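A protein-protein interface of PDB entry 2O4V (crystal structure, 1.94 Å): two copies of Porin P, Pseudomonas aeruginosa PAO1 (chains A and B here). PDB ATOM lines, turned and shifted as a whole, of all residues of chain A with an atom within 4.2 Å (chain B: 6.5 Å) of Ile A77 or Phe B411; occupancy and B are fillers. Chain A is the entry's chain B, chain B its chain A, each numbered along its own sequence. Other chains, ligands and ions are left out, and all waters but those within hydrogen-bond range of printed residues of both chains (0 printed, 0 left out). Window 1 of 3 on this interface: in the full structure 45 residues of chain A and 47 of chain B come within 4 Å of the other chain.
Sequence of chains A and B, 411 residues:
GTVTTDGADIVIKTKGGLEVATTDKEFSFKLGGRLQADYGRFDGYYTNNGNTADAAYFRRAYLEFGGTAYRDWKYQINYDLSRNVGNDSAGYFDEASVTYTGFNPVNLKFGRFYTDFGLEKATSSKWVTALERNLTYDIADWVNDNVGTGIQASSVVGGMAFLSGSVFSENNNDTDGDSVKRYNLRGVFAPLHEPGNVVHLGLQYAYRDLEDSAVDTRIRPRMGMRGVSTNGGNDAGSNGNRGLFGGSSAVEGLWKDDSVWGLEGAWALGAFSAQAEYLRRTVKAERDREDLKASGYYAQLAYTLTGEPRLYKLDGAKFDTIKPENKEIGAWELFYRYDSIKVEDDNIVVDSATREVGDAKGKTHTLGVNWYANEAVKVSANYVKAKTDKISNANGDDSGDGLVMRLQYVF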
ATOM      1  N   LEU A  63      20.808  11.955 -34.007  1.00  0.00           N
ATOM      2  CA  LEU A  63      21.436  13.131 -34.590  1.00  0.00           C
ATOM      3  C   LEU A  63      22.764  13.311 -33.866  1.00  0.00           C
ATOM      4  O   LEU A  63      22.828  13.214 -32.630  1.00  0.00           O
ATOM      5  CB  LEU A  63      20.562  14.368 -34.434  1.00  0.00           C
ATOM      6  CG  LEU A  63      19.212  14.376 -35.158  1.00  0.00           C
ATOM      7  CD1 LEU A  63      18.466  15.654 -34.809  1.00  0.00           C
ATOM      8  CD2 LEU A  63      19.356  14.210 -36.684  1.00  0.00           C
ATOM      9  N   GLU A  64      23.811  13.554 -34.648  1.00  0.00           N
ATOM     10  CA  GLU A  64      25.191  13.488 -34.179  1.00  0.00           C
ATOM     11  C   GLU A  64      25.926  14.782 -34.499  1.00  0.00           C
ATOM     12  O   GLU A  64      26.051  15.166 -35.668  1.00  0.00           O
ATOM     13  CB  GLU A  64      25.895  12.275 -34.812  1.00  0.00           C
ATOM     14  CG  GLU A  64      25.194  10.925 -34.477  1.00  0.00           C
ATOM     15  CD  GLU A  64      25.675   9.765 -35.339  1.00  0.00           C
ATOM     16  OE1 GLU A  64      26.818   9.812 -35.842  1.00  0.00           O
ATOM     17  OE2 GLU A  64      24.904   8.797 -35.518  1.00  0.00           O
ATOM     18  N   PHE A  65      26.375  15.468 -33.452  1.00  0.00           N
ATOM     19  CA  PHE A  65      27.133  16.715 -33.590  1.00  0.00           C
ATOM     20  C   PHE A  65      28.477  16.541 -32.894  1.00  0.00           C
ATOM     21  O   PHE A  65      28.547  16.193 -31.705  1.00  0.00           O
ATOM     22  CB  PHE A  65      26.372  17.908 -32.997  1.00  0.00           C
ATOM     23  CG  PHE A  65      24.938  18.009 -33.460  1.00  0.00           C
ATOM     24  CD1 PHE A  65      24.577  18.943 -34.423  1.00  0.00           C
ATOM     25  CD2 PHE A  65      23.958  17.161 -32.942  1.00  0.00           C
ATOM     26  CE1 PHE A  65      23.254  19.034 -34.868  1.00  0.00           C
ATOM     27  CE2 PHE A  65      22.631  17.244 -33.375  1.00  0.00           C
ATOM     28  CZ  PHE A  65      22.284  18.185 -34.344  1.00  0.00           C
ATOM     29  N   TYR A  75      34.582  17.397 -28.999  1.00  0.00           N
ATOM     30  CA  TYR A  75      33.300  17.064 -28.383  1.00  0.00           C
ATOM     31  C   TYR A  75      32.514  16.144 -29.311  1.00  0.00           C
ATOM     32  O   TYR A  75      32.742  16.132 -30.531  1.00  0.00           O
ATOM     33  CB  TYR A  75      32.493  18.324 -28.057  1.00  0.00           C
ATOM     34  CG  TYR A  75      31.833  18.971 -29.255  1.00  0.00           C
ATOM     35  CD1 TYR A  75      32.527  19.873 -30.058  1.00  0.00           C
ATOM     36  CD2 TYR A  75      30.515  18.672 -29.591  1.00  0.00           C
ATOM     37  CE1 TYR A  75      31.918  20.470 -31.167  1.00  0.00           C
ATOM     38  CE2 TYR A  75      29.899  19.259 -30.695  1.00  0.00           C
ATOM     39  CZ  TYR A  75      30.605  20.151 -31.479  1.00  0.00           C
ATOM     40  OH  TYR A  75      29.989  20.735 -32.568  1.00  0.00           O
ATOM     41  N   GLN A  76      31.597  15.385 -28.720  1.00  0.00           N
ATOM     42  CA  GLN A  76      30.650  14.549 -29.465  1.00  0.00           C
ATOM     43  C   GLN A  76      29.335  14.459 -28.702  1.00  0.00           C
ATOM     44  O   GLN A  76      29.299  13.947 -27.576  1.00  0.00           O
ATOM     45  CB  GLN A  76      31.216  13.142 -29.710  1.00  0.00           C
ATOM     46  CG  GLN A  76      30.384  12.298 -30.702  1.00  0.00           C
ATOM     47  CD  GLN A  76      30.457  12.833 -32.130  1.00  0.00           C
ATOM     48  OE1 GLN A  76      31.536  13.144 -32.632  1.00  0.00           O
ATOM     49  NE2 GLN A  76      29.310  12.939 -32.788  1.00  0.00           N
ATOM     50  N   ILE A  77      28.267  14.966 -29.315  1.00  0.00           N
ATOM     51  CA  ILE A  77      26.915  14.894 -28.749  1.00  0.00           C
ATOM     52  C   ILE A  77      25.979  14.143 -29.703  1.00  0.00           C
ATOM     53  O   ILE A  77      25.598  14.664 -30.756  1.00  0.00           O
ATOM     54  CB  ILE A  77      26.344  16.304 -28.424  1.00  0.00           C
ATOM     55  CG1 ILE A  77      27.297  17.071 -27.496  1.00  0.00           C
ATOM     56  CG2 ILE A  77      24.929  16.195 -27.802  1.00  0.00           C
ATOM     57  CD1 ILE A  77      27.074  18.587 -27.466  1.00  0.00           C
ATOM     58  N   ASN A  78      25.632  12.912 -29.327  1.00  0.00           N
ATOM     59  CA  ASN A  78      24.703  12.078 -30.085  1.00  0.00           C
ATOM     60  C   ASN A  78      23.388  11.913 -29.328  1.00  0.00           C
ATOM     61  O   ASN A  78      23.379  11.368 -28.220  1.00  0.00           O
ATOM     62  CB  ASN A  78      25.307  10.697 -30.336  1.00  0.00           C
ATOM     63  CG  ASN A  78      26.610  10.750 -31.133  1.00  0.00           C
ATOM     64  OD1 ASN A  78      26.984  11.787 -31.689  1.00  0.00           O
ATOM     65  ND2 ASN A  78      27.296   9.612 -31.203  1.00  0.00           N
ATOM     66  N   TYR A  79      22.284  12.382 -29.915  1.00  0.00           N
ATOM     67  CA  TYR A  79      20.976  12.285 -29.254  1.00  0.00           C
ATOM     68  C   TYR A  79      20.046  11.293 -29.953  1.00  0.00           C
ATOM     69  O   TYR A  79      19.905  11.322 -31.178  1.00  0.00           O
ATOM     70  CB  TYR A  79      20.314  13.664 -29.135  1.00  0.00           C
ATOM     71  CG  TYR A  79      19.541  13.841 -27.838  1.00  0.00           C
ATOM     72  CD1 TYR A  79      20.218  13.883 -26.606  1.00  0.00           C
ATOM     73  CD2 TYR A  79      18.145  13.955 -27.832  1.00  0.00           C
ATOM     74  CE1 TYR A  79      19.533  14.040 -25.402  1.00  0.00           C
ATOM     75  CE2 TYR A  79      17.441  14.115 -26.620  1.00  0.00           C
ATOM     76  CZ  TYR A  79      18.147  14.166 -25.411  1.00  0.00           C
ATOM     77  OH  TYR A  79      17.489  14.323 -24.195  1.00  0.00           O
ATOM     78  N   GLU A  95      25.692   9.666 -26.678  1.00  0.00           N
ATOM     79  CA  GLU A  95      26.963  10.195 -26.193  1.00  0.00           C
ATOM     80  C   GLU A  95      26.867  11.695 -25.945  1.00  0.00           C
ATOM     81  O   GLU A  95      26.156  12.410 -26.648  1.00  0.00           O
ATOM     82  CB  GLU A  95      28.105   9.893 -27.192  1.00  0.00           C
ATOM     83  CG  GLU A  95      29.497  10.343 -26.731  1.00  0.00           C
ATOM     84  CD  GLU A  95      30.619   9.855 -27.641  1.00  0.00           C
ATOM     85  OE1 GLU A  95      30.334   9.187 -28.666  1.00  0.00           O
ATOM     86  OE2 GLU A  95      31.797  10.143 -27.332  1.00  0.00           O
ATOM     87  N   LYS B  15      34.590  27.161 -35.354  1.00  0.00           N
ATOM     88  CA  LYS B  15      35.430  27.018 -34.170  1.00  0.00           C
ATOM     89  C   LYS B  15      34.963  25.791 -33.376  1.00  0.00           C
ATOM     90  O   LYS B  15      35.077  25.743 -32.157  1.00  0.00           O
ATOM     91  CB  LYS B  15      35.396  28.296 -33.319  1.00  0.00           C
ATOM     92  CG  LYS B  15      35.998  29.540 -33.991  1.00  0.00           C
ATOM     93  CD  LYS B  15      37.436  29.756 -33.570  1.00  0.00           C
ATOM     94  CE  LYS B  15      37.981  31.115 -34.013  1.00  0.00           C
ATOM     95  NZ  LYS B  15      38.397  31.133 -35.448  1.00  0.00           N
ATOM     96  N   GLY B  16      34.453  24.792 -34.096  1.00  0.00           N
ATOM     97  CA  GLY B  16      33.823  23.617 -33.488  1.00  0.00           C
ATOM     98  C   GLY B  16      32.353  23.510 -33.860  1.00  0.00           C
ATOM     99  O   GLY B  16      31.770  22.420 -33.834  1.00  0.00           O
ATOM    100  N   GLY B  17      31.749  24.651 -34.184  1.00  0.00           N
ATOM    101  CA  GLY B  17      30.371  24.716 -34.663  1.00  0.00           C
ATOM    102  C   GLY B  17      30.371  25.197 -36.094  1.00  0.00           C
ATOM    103  O   GLY B  17      31.319  24.936 -36.837  1.00  0.00           O
ATOM    104  N   LEU B  18      29.323  25.911 -36.495  1.00  0.00           N
ATOM    105  CA  LEU B  18      29.273  26.436 -37.862  1.00  0.00           C
ATOM    106  C   LEU B  18      28.566  27.781 -37.970  1.00  0.00           C
ATOM    107  O   LEU B  18      27.531  28.004 -37.341  1.00  0.00           O
ATOM    108  CB  LEU B  18      28.609  25.410 -38.797  1.00  0.00           C
ATOM    109  CG  LEU B  18      28.586  25.737 -40.295  1.00  0.00           C
ATOM    110  CD1 LEU B  18      29.986  25.723 -40.902  1.00  0.00           C
ATOM    111  CD2 LEU B  18      27.662  24.750 -41.004  1.00  0.00           C
ATOM    112  N   LYS B  30      23.710  30.053 -37.935  1.00  0.00           N
ATOM    113  CA  LYS B  30      24.703  29.701 -36.933  1.00  0.00           C
ATOM    114  C   LYS B  30      24.234  28.484 -36.144  1.00  0.00           C
ATOM    115  O   LYS B  30      23.142  28.488 -35.538  1.00  0.00           O
ATOM    116  CB  LYS B  30      24.989  30.894 -36.012  1.00  0.00           C
ATOM    117  CG  LYS B  30      25.934  30.604 -34.844  1.00  0.00           C
ATOM    118  CD  LYS B  30      26.311  31.902 -34.124  1.00  0.00           C
ATOM    119  CE  LYS B  30      27.130  31.630 -32.872  1.00  0.00           C
ATOM    120  NZ  LYS B  30      28.490  31.071 -33.183  1.00  0.00           N
ATOM    121  N   LEU B  31      25.054  27.438 -36.177  1.00  0.00           N
ATOM    122  CA  LEU B  31      24.825  26.248 -35.368  1.00  0.00           C
ATOM    123  C   LEU B  31      25.897  26.200 -34.294  1.00  0.00           C
ATOM    124  O   LEU B  31      27.093  26.203 -34.594  1.00  0.00           O
ATOM    125  CB  LEU B  31      24.859  24.973 -36.236  1.00  0.00           C
ATOM    126  CG  LEU B  31      24.442  23.627 -35.626  1.00  0.00           C
ATOM    127  CD1 LEU B  31      24.188  22.630 -36.740  1.00  0.00           C
ATOM    128  CD2 LEU B  31      25.505  23.081 -34.666  1.00  0.00           C
ATOM    129  N   GLY B  32      25.461  26.162 -33.039  1.00  0.00           N
ATOM    130  CA  GLY B  32      26.379  26.091 -31.924  1.00  0.00           C
ATOM    131  C   GLY B  32      25.785  25.292 -30.792  1.00  0.00           C
ATOM    132  O   GLY B  32      24.783  24.586 -30.967  1.00  0.00           O
ATOM    133  N   GLY B  33      26.401  25.403 -29.627  1.00  0.00           N
ATOM    134  CA  GLY B  33      25.889  24.713 -28.458  1.00  0.00           C
ATOM    135  C   GLY B  33      26.754  24.925 -27.245  1.00  0.00           C
ATOM    136  O   GLY B  33      27.735  25.689 -27.285  1.00  0.00           O
ATOM    137  N   ARG B  34      26.372  24.270 -26.153  1.00  0.00           N
ATOM    138  CA  ARG B  34      27.149  24.311 -24.921  1.00  0.00           C
ATOM    139  C   ARG B  34      26.925  23.029 -24.137  1.00  0.00           C
ATOM    140  O   ARG B  34      25.797  22.536 -24.032  1.00  0.00           O
ATOM    141  CB  ARG B  34      26.827  25.558 -24.075  1.00  0.00           C
ATOM    142  CG  ARG B  34      25.448  25.567 -23.359  1.00  0.00           C
ATOM    143  CD  ARG B  34      25.059  26.973 -22.934  1.00  0.00           C
ATOM    144  NE  ARG B  34      24.705  27.811 -24.085  1.00  0.00           N
ATOM    145  CZ  ARG B  34      24.206  29.039 -23.996  1.00  0.00           C
ATOM    146  NH1 ARG B  34      23.908  29.722 -25.098  1.00  0.00           N
ATOM    147  NH2 ARG B  34      24.008  29.595 -22.805  1.00  0.00           N
ATOM    148  N   LEU B  35      28.012  22.477 -23.617  1.00  0.00           N
ATOM    149  CA  LEU B  35      27.954  21.300 -22.773  1.00  0.00           C
ATOM    150  C   LEU B  35      28.596  21.663 -21.440  1.00  0.00           C
ATOM    151  O   LEU B  35      29.730  22.109 -21.406  1.00  0.00           O
ATOM    152  CB  LEU B  35      28.699  20.130 -23.429  1.00  0.00           C
ATOM    153  CG  LEU B  35      28.479  18.715 -22.883  1.00  0.00           C
ATOM    154  CD1 LEU B  35      26.983  18.338 -22.898  1.00  0.00           C
ATOM    155  CD2 LEU B  35      29.300  17.692 -23.676  1.00  0.00           C
ATOM    156  N   ALA B  61      22.989  21.084 -21.769  1.00  0.00           N
ATOM    157  CA  ALA B  61      23.487  20.473 -23.000  1.00  0.00           C
ATOM    158  C   ALA B  61      22.630  21.033 -24.120  1.00  0.00           C
ATOM    159  O   ALA B  61      21.657  20.407 -24.533  1.00  0.00           O
ATOM    160  CB  ALA B  61      23.385  18.940 -22.940  1.00  0.00           C
ATOM    161  N   TYR B  62      22.956  22.243 -24.570  1.00  0.00           N
ATOM    162  CA  TYR B  62      22.133  22.913 -25.575  1.00  0.00           C
ATOM    163  C   TYR B  62      22.656  22.674 -26.977  1.00  0.00           C
ATOM    164  O   TYR B  62      23.863  22.735 -27.215  1.00  0.00           O
ATOM    165  CB  TYR B  62      22.090  24.433 -25.381  1.00  0.00           C
ATOM    166  CG  TYR B  62      21.578  24.996 -24.065  1.00  0.00           C
ATOM    167  CD1 TYR B  62      20.974  24.196 -23.100  1.00  0.00           C
ATOM    168  CD2 TYR B  62      21.657  26.367 -23.829  1.00  0.00           C
ATOM    169  CE1 TYR B  62      20.507  24.752 -21.899  1.00  0.00           C
ATOM    170  CE2 TYR B  62      21.203  26.928 -22.645  1.00  0.00           C
ATOM    171  CZ  TYR B  62      20.631  26.124 -21.693  1.00  0.00           C
ATOM    172  OH  TYR B  62      20.176  26.700 -20.534  1.00  0.00           O
ATOM    173  N   LEU B  63      21.733  22.420 -27.895  1.00  0.00           N
ATOM    174  CA  LEU B  63      21.992  22.586 -29.312  1.00  0.00           C
ATOM    175  C   LEU B  63      21.306  23.883 -29.698  1.00  0.00           C
ATOM    176  O   LEU B  63      20.157  24.140 -29.297  1.00  0.00           O
ATOM    177  CB  LEU B  63      21.462  21.403 -30.131  1.00  0.00           C
ATOM    178  CG  LEU B  63      22.030  20.024 -29.756  1.00  0.00           C
ATOM    179  CD1 LEU B  63      21.373  18.922 -30.589  1.00  0.00           C
ATOM    180  CD2 LEU B  63      23.550  19.961 -29.890  1.00  0.00           C
ATOM    181  N   GLU B  64      22.023  24.705 -30.449  1.00  0.00           N
ATOM    182  CA  GLU B  64      21.629  26.083 -30.683  1.00  0.00           C
ATOM    183  C   GLU B  64      21.565  26.380 -32.173  1.00  0.00           C
ATOM    184  O   GLU B  64      22.569  26.248 -32.892  1.00  0.00           O
ATOM    185  CB  GLU B  64      22.597  27.039 -29.954  1.00  0.00           C
ATOM    186  CG  GLU B  64      22.642  26.807 -28.432  1.00  0.00           C
ATOM    187  CD  GLU B  64      23.790  27.522 -27.720  1.00  0.00           C
ATOM    188  OE1 GLU B  64      24.277  28.565 -28.201  1.00  0.00           O
ATOM    189  OE2 GLU B  64      24.213  27.032 -26.656  1.00  0.00           O
ATOM    190  N   LEU B  81      19.022  19.320 -24.126  1.00  0.00           N
ATOM    191  CA  LEU B  81      19.060  17.863 -24.103  1.00  0.00           C
ATOM    192  C   LEU B  81      19.237  17.303 -22.683  1.00  0.00           C
ATOM    193  O   LEU B  81      18.933  16.141 -22.435  1.00  0.00           O
ATOM    194  CB  LEU B  81      20.196  17.352 -25.021  1.00  0.00           C
ATOM    195  CG  LEU B  81      20.301  17.903 -26.450  1.00  0.00           C
ATOM    196  CD1 LEU B  81      21.405  17.172 -27.225  1.00  0.00           C
ATOM    197  CD2 LEU B  81      18.983  17.829 -27.196  1.00  0.00           C
ATOM    198  N   LYS B 126      26.836  30.544 -20.425  1.00  0.00           N
ATOM    199  CA  LYS B 126      28.211  30.183 -20.774  1.00  0.00           C
ATOM    200  C   LYS B 126      29.217  30.930 -19.909  1.00  0.00           C
ATOM    201  O   LYS B 126      30.255  30.370 -19.538  1.00  0.00           O
ATOM    202  CB  LYS B 126      28.492  30.455 -22.253  1.00  0.00           C
ATOM    203  CG  LYS B 126      27.698  29.566 -23.196  1.00  0.00           C
ATOM    204  CD  LYS B 126      28.138  29.731 -24.645  1.00  0.00           C
ATOM    205  CE  LYS B 126      27.511  30.949 -25.306  1.00  0.00           C
ATOM    206  NZ  LYS B 126      27.815  30.951 -26.770  1.00  0.00           N
ATOM    207  N   ALA B 376      36.755  28.039 -26.310  1.00  0.00           N
ATOM    208  CA  ALA B 376      35.800  26.928 -26.327  1.00  0.00           C
ATOM    209  C   ALA B 376      35.663  26.240 -24.967  1.00  0.00           C
ATOM    210  O   ALA B 376      34.562  25.851 -24.579  1.00  0.00           O
ATOM    211  CB  ALA B 376      36.184  25.906 -27.399  1.00  0.00           C
ATOM    212  N   TYR B 409      32.291  23.042 -22.556  1.00  0.00           N
ATOM    213  CA  TYR B 409      32.743  23.138 -23.933  1.00  0.00           C
ATOM    214  C   TYR B 409      31.656  23.887 -24.698  1.00  0.00           C
ATOM    215  O   TYR B 409      30.488  23.492 -24.682  1.00  0.00           O
ATOM    216  CB  TYR B 409      32.974  21.736 -24.507  1.00  0.00           C
ATOM    217  CG  TYR B 409      33.739  21.666 -25.820  1.00  0.00           C
ATOM    218  CD1 TYR B 409      34.862  20.843 -25.948  1.00  0.00           C
ATOM    219  CD2 TYR B 409      33.323  22.391 -26.950  1.00  0.00           C
ATOM    220  CE1 TYR B 409      35.560  20.758 -27.162  1.00  0.00           C
ATOM    221  CE2 TYR B 409      34.029  22.320 -28.163  1.00  0.00           C
ATOM    222  CZ  TYR B 409      35.133  21.496 -28.258  1.00  0.00           C
ATOM    223  OH  TYR B 409      35.808  21.414 -29.450  1.00  0.00           O
ATOM    224  N   VAL B 410      32.035  24.989 -25.336  1.00  0.00           N
ATOM    225  CA  VAL B 410      31.085  25.766 -26.142  1.00  0.00           C
ATOM    226  C   VAL B 410      31.498  25.761 -27.613  1.00  0.00           C
ATOM    227  O   VAL B 410      32.694  25.747 -27.929  1.00  0.00           O
ATOM    228  CB  VAL B 410      30.878  27.211 -25.588  1.00  0.00           C
ATOM    229  CG1 VAL B 410      30.373  27.166 -24.135  1.00  0.00           C
ATOM    230  CG2 VAL B 410      32.153  28.015 -25.653  1.00  0.00           C
ATOM    231  N   PHE B 411      30.518  25.747 -28.511  1.00  0.00           N
ATOM    232  CA  PHE B 411      30.824  25.751 -29.950  1.00  0.00           C
ATOM    233  C   PHE B 411      29.812  26.582 -30.737  1.00  0.00           C
ATOM    234  O   PHE B 411      28.799  27.006 -30.173  1.00  0.00           O
ATOM    235  CB  PHE B 411      30.964  24.317 -30.498  1.00  0.00           C
ATOM    236  CG  PHE B 411      29.757  23.460 -30.273  1.00  0.00           C
ATOM    237  CD1 PHE B 411      29.551  22.811 -29.043  1.00  0.00           C
ATOM    238  CD2 PHE B 411      28.817  23.294 -31.284  1.00  0.00           C
ATOM    239  CE1 PHE B 411      28.417  22.017 -28.841  1.00  0.00           C
ATOM    240  CE2 PHE B 411      27.691  22.496 -31.091  1.00  0.00           C
ATOM    241  CZ  PHE B 411      27.485  21.866 -29.866  1.00  0.00           C
ATOM    242  OXT PHE B 411      29.996  26.892 -31.925  1.00  0.00           O
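The backbone carbonyl oxygen of Gly B16 is in hydrogen-bond range of the side-chain hydroxyl of Tyr A75 (2.8 Å).
O of Leu B81 lies within hydrogen-bond range of OH of Tyr A79.
The backbone NH of Gly B33 is in hydrogen-bond range of the chain-end carboxylate of Phe B411, at 2.9 Å.
O of Tyr B409 sits at hydrogen-bond distance from N of Leu B35.
The backbone carbonyl oxygen (O) of Ala B61 lies within hydrogen-bond range of the backbone NH (N) of Leu B81, 2.9 Å away.
The backbone carbonyl oxygen (O) of Leu A63 lies within hydrogen-bond range of the backbone NH (N) of Tyr A79 (2.9 Å).
N of Ile A77 is in hydrogen-bond range of O of Phe A65 (2.7 Å).
Among the printed residues, pairs that only touch across the chains: Phe A65 with Leu B63 (3.5 Å), Tyr A75 with Tyr B409 (3.4 Å), Tyr A75 with Phe B411 (3.1 Å), Ile A77 with Leu B81 (3.7 Å) and Ile A77 with Phe B411 (3.9 Å).
Ile A77 touches just these residues of chain B: Leu B81 (3.7 Å) and Phe B411 (3.9 Å).
Of the printed residues of chain B, Phe A65 touches Leu B63.
Of the printed residues of chain A, Leu B81 touches Ile A77 (3.7 Å) and Tyr A79 (2.9 Å).
Of the printed residues of chain A, Tyr B409 touches Tyr A75 (3.4 Å).
Of the printed residues of chain B, Tyr A79 touches Leu B81.
Printed residues of chain A within 4 Å of Leu B63: Phe A65 (3.5 Å).
Glu B64 touches none of the printed residues of chain A.
The nearest printed residue of chain B that does not touch Tyr A75 is Gly B17 (4.5 Å).
Printed residues of chain A that touch a printed residue of chain B: Phe A65, Tyr A75, Ile A77 and Tyr A79.
Of the 20 printed residues of chain B, 5 touch a printed residue of chain A.
Hydrophobic or aromatic side chains of chain B within 4 Å of the printed part of chain A: Leu B63, Leu B81, Tyr B409 and Phe B411.
Positions printed for both chains: 63 and 64.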
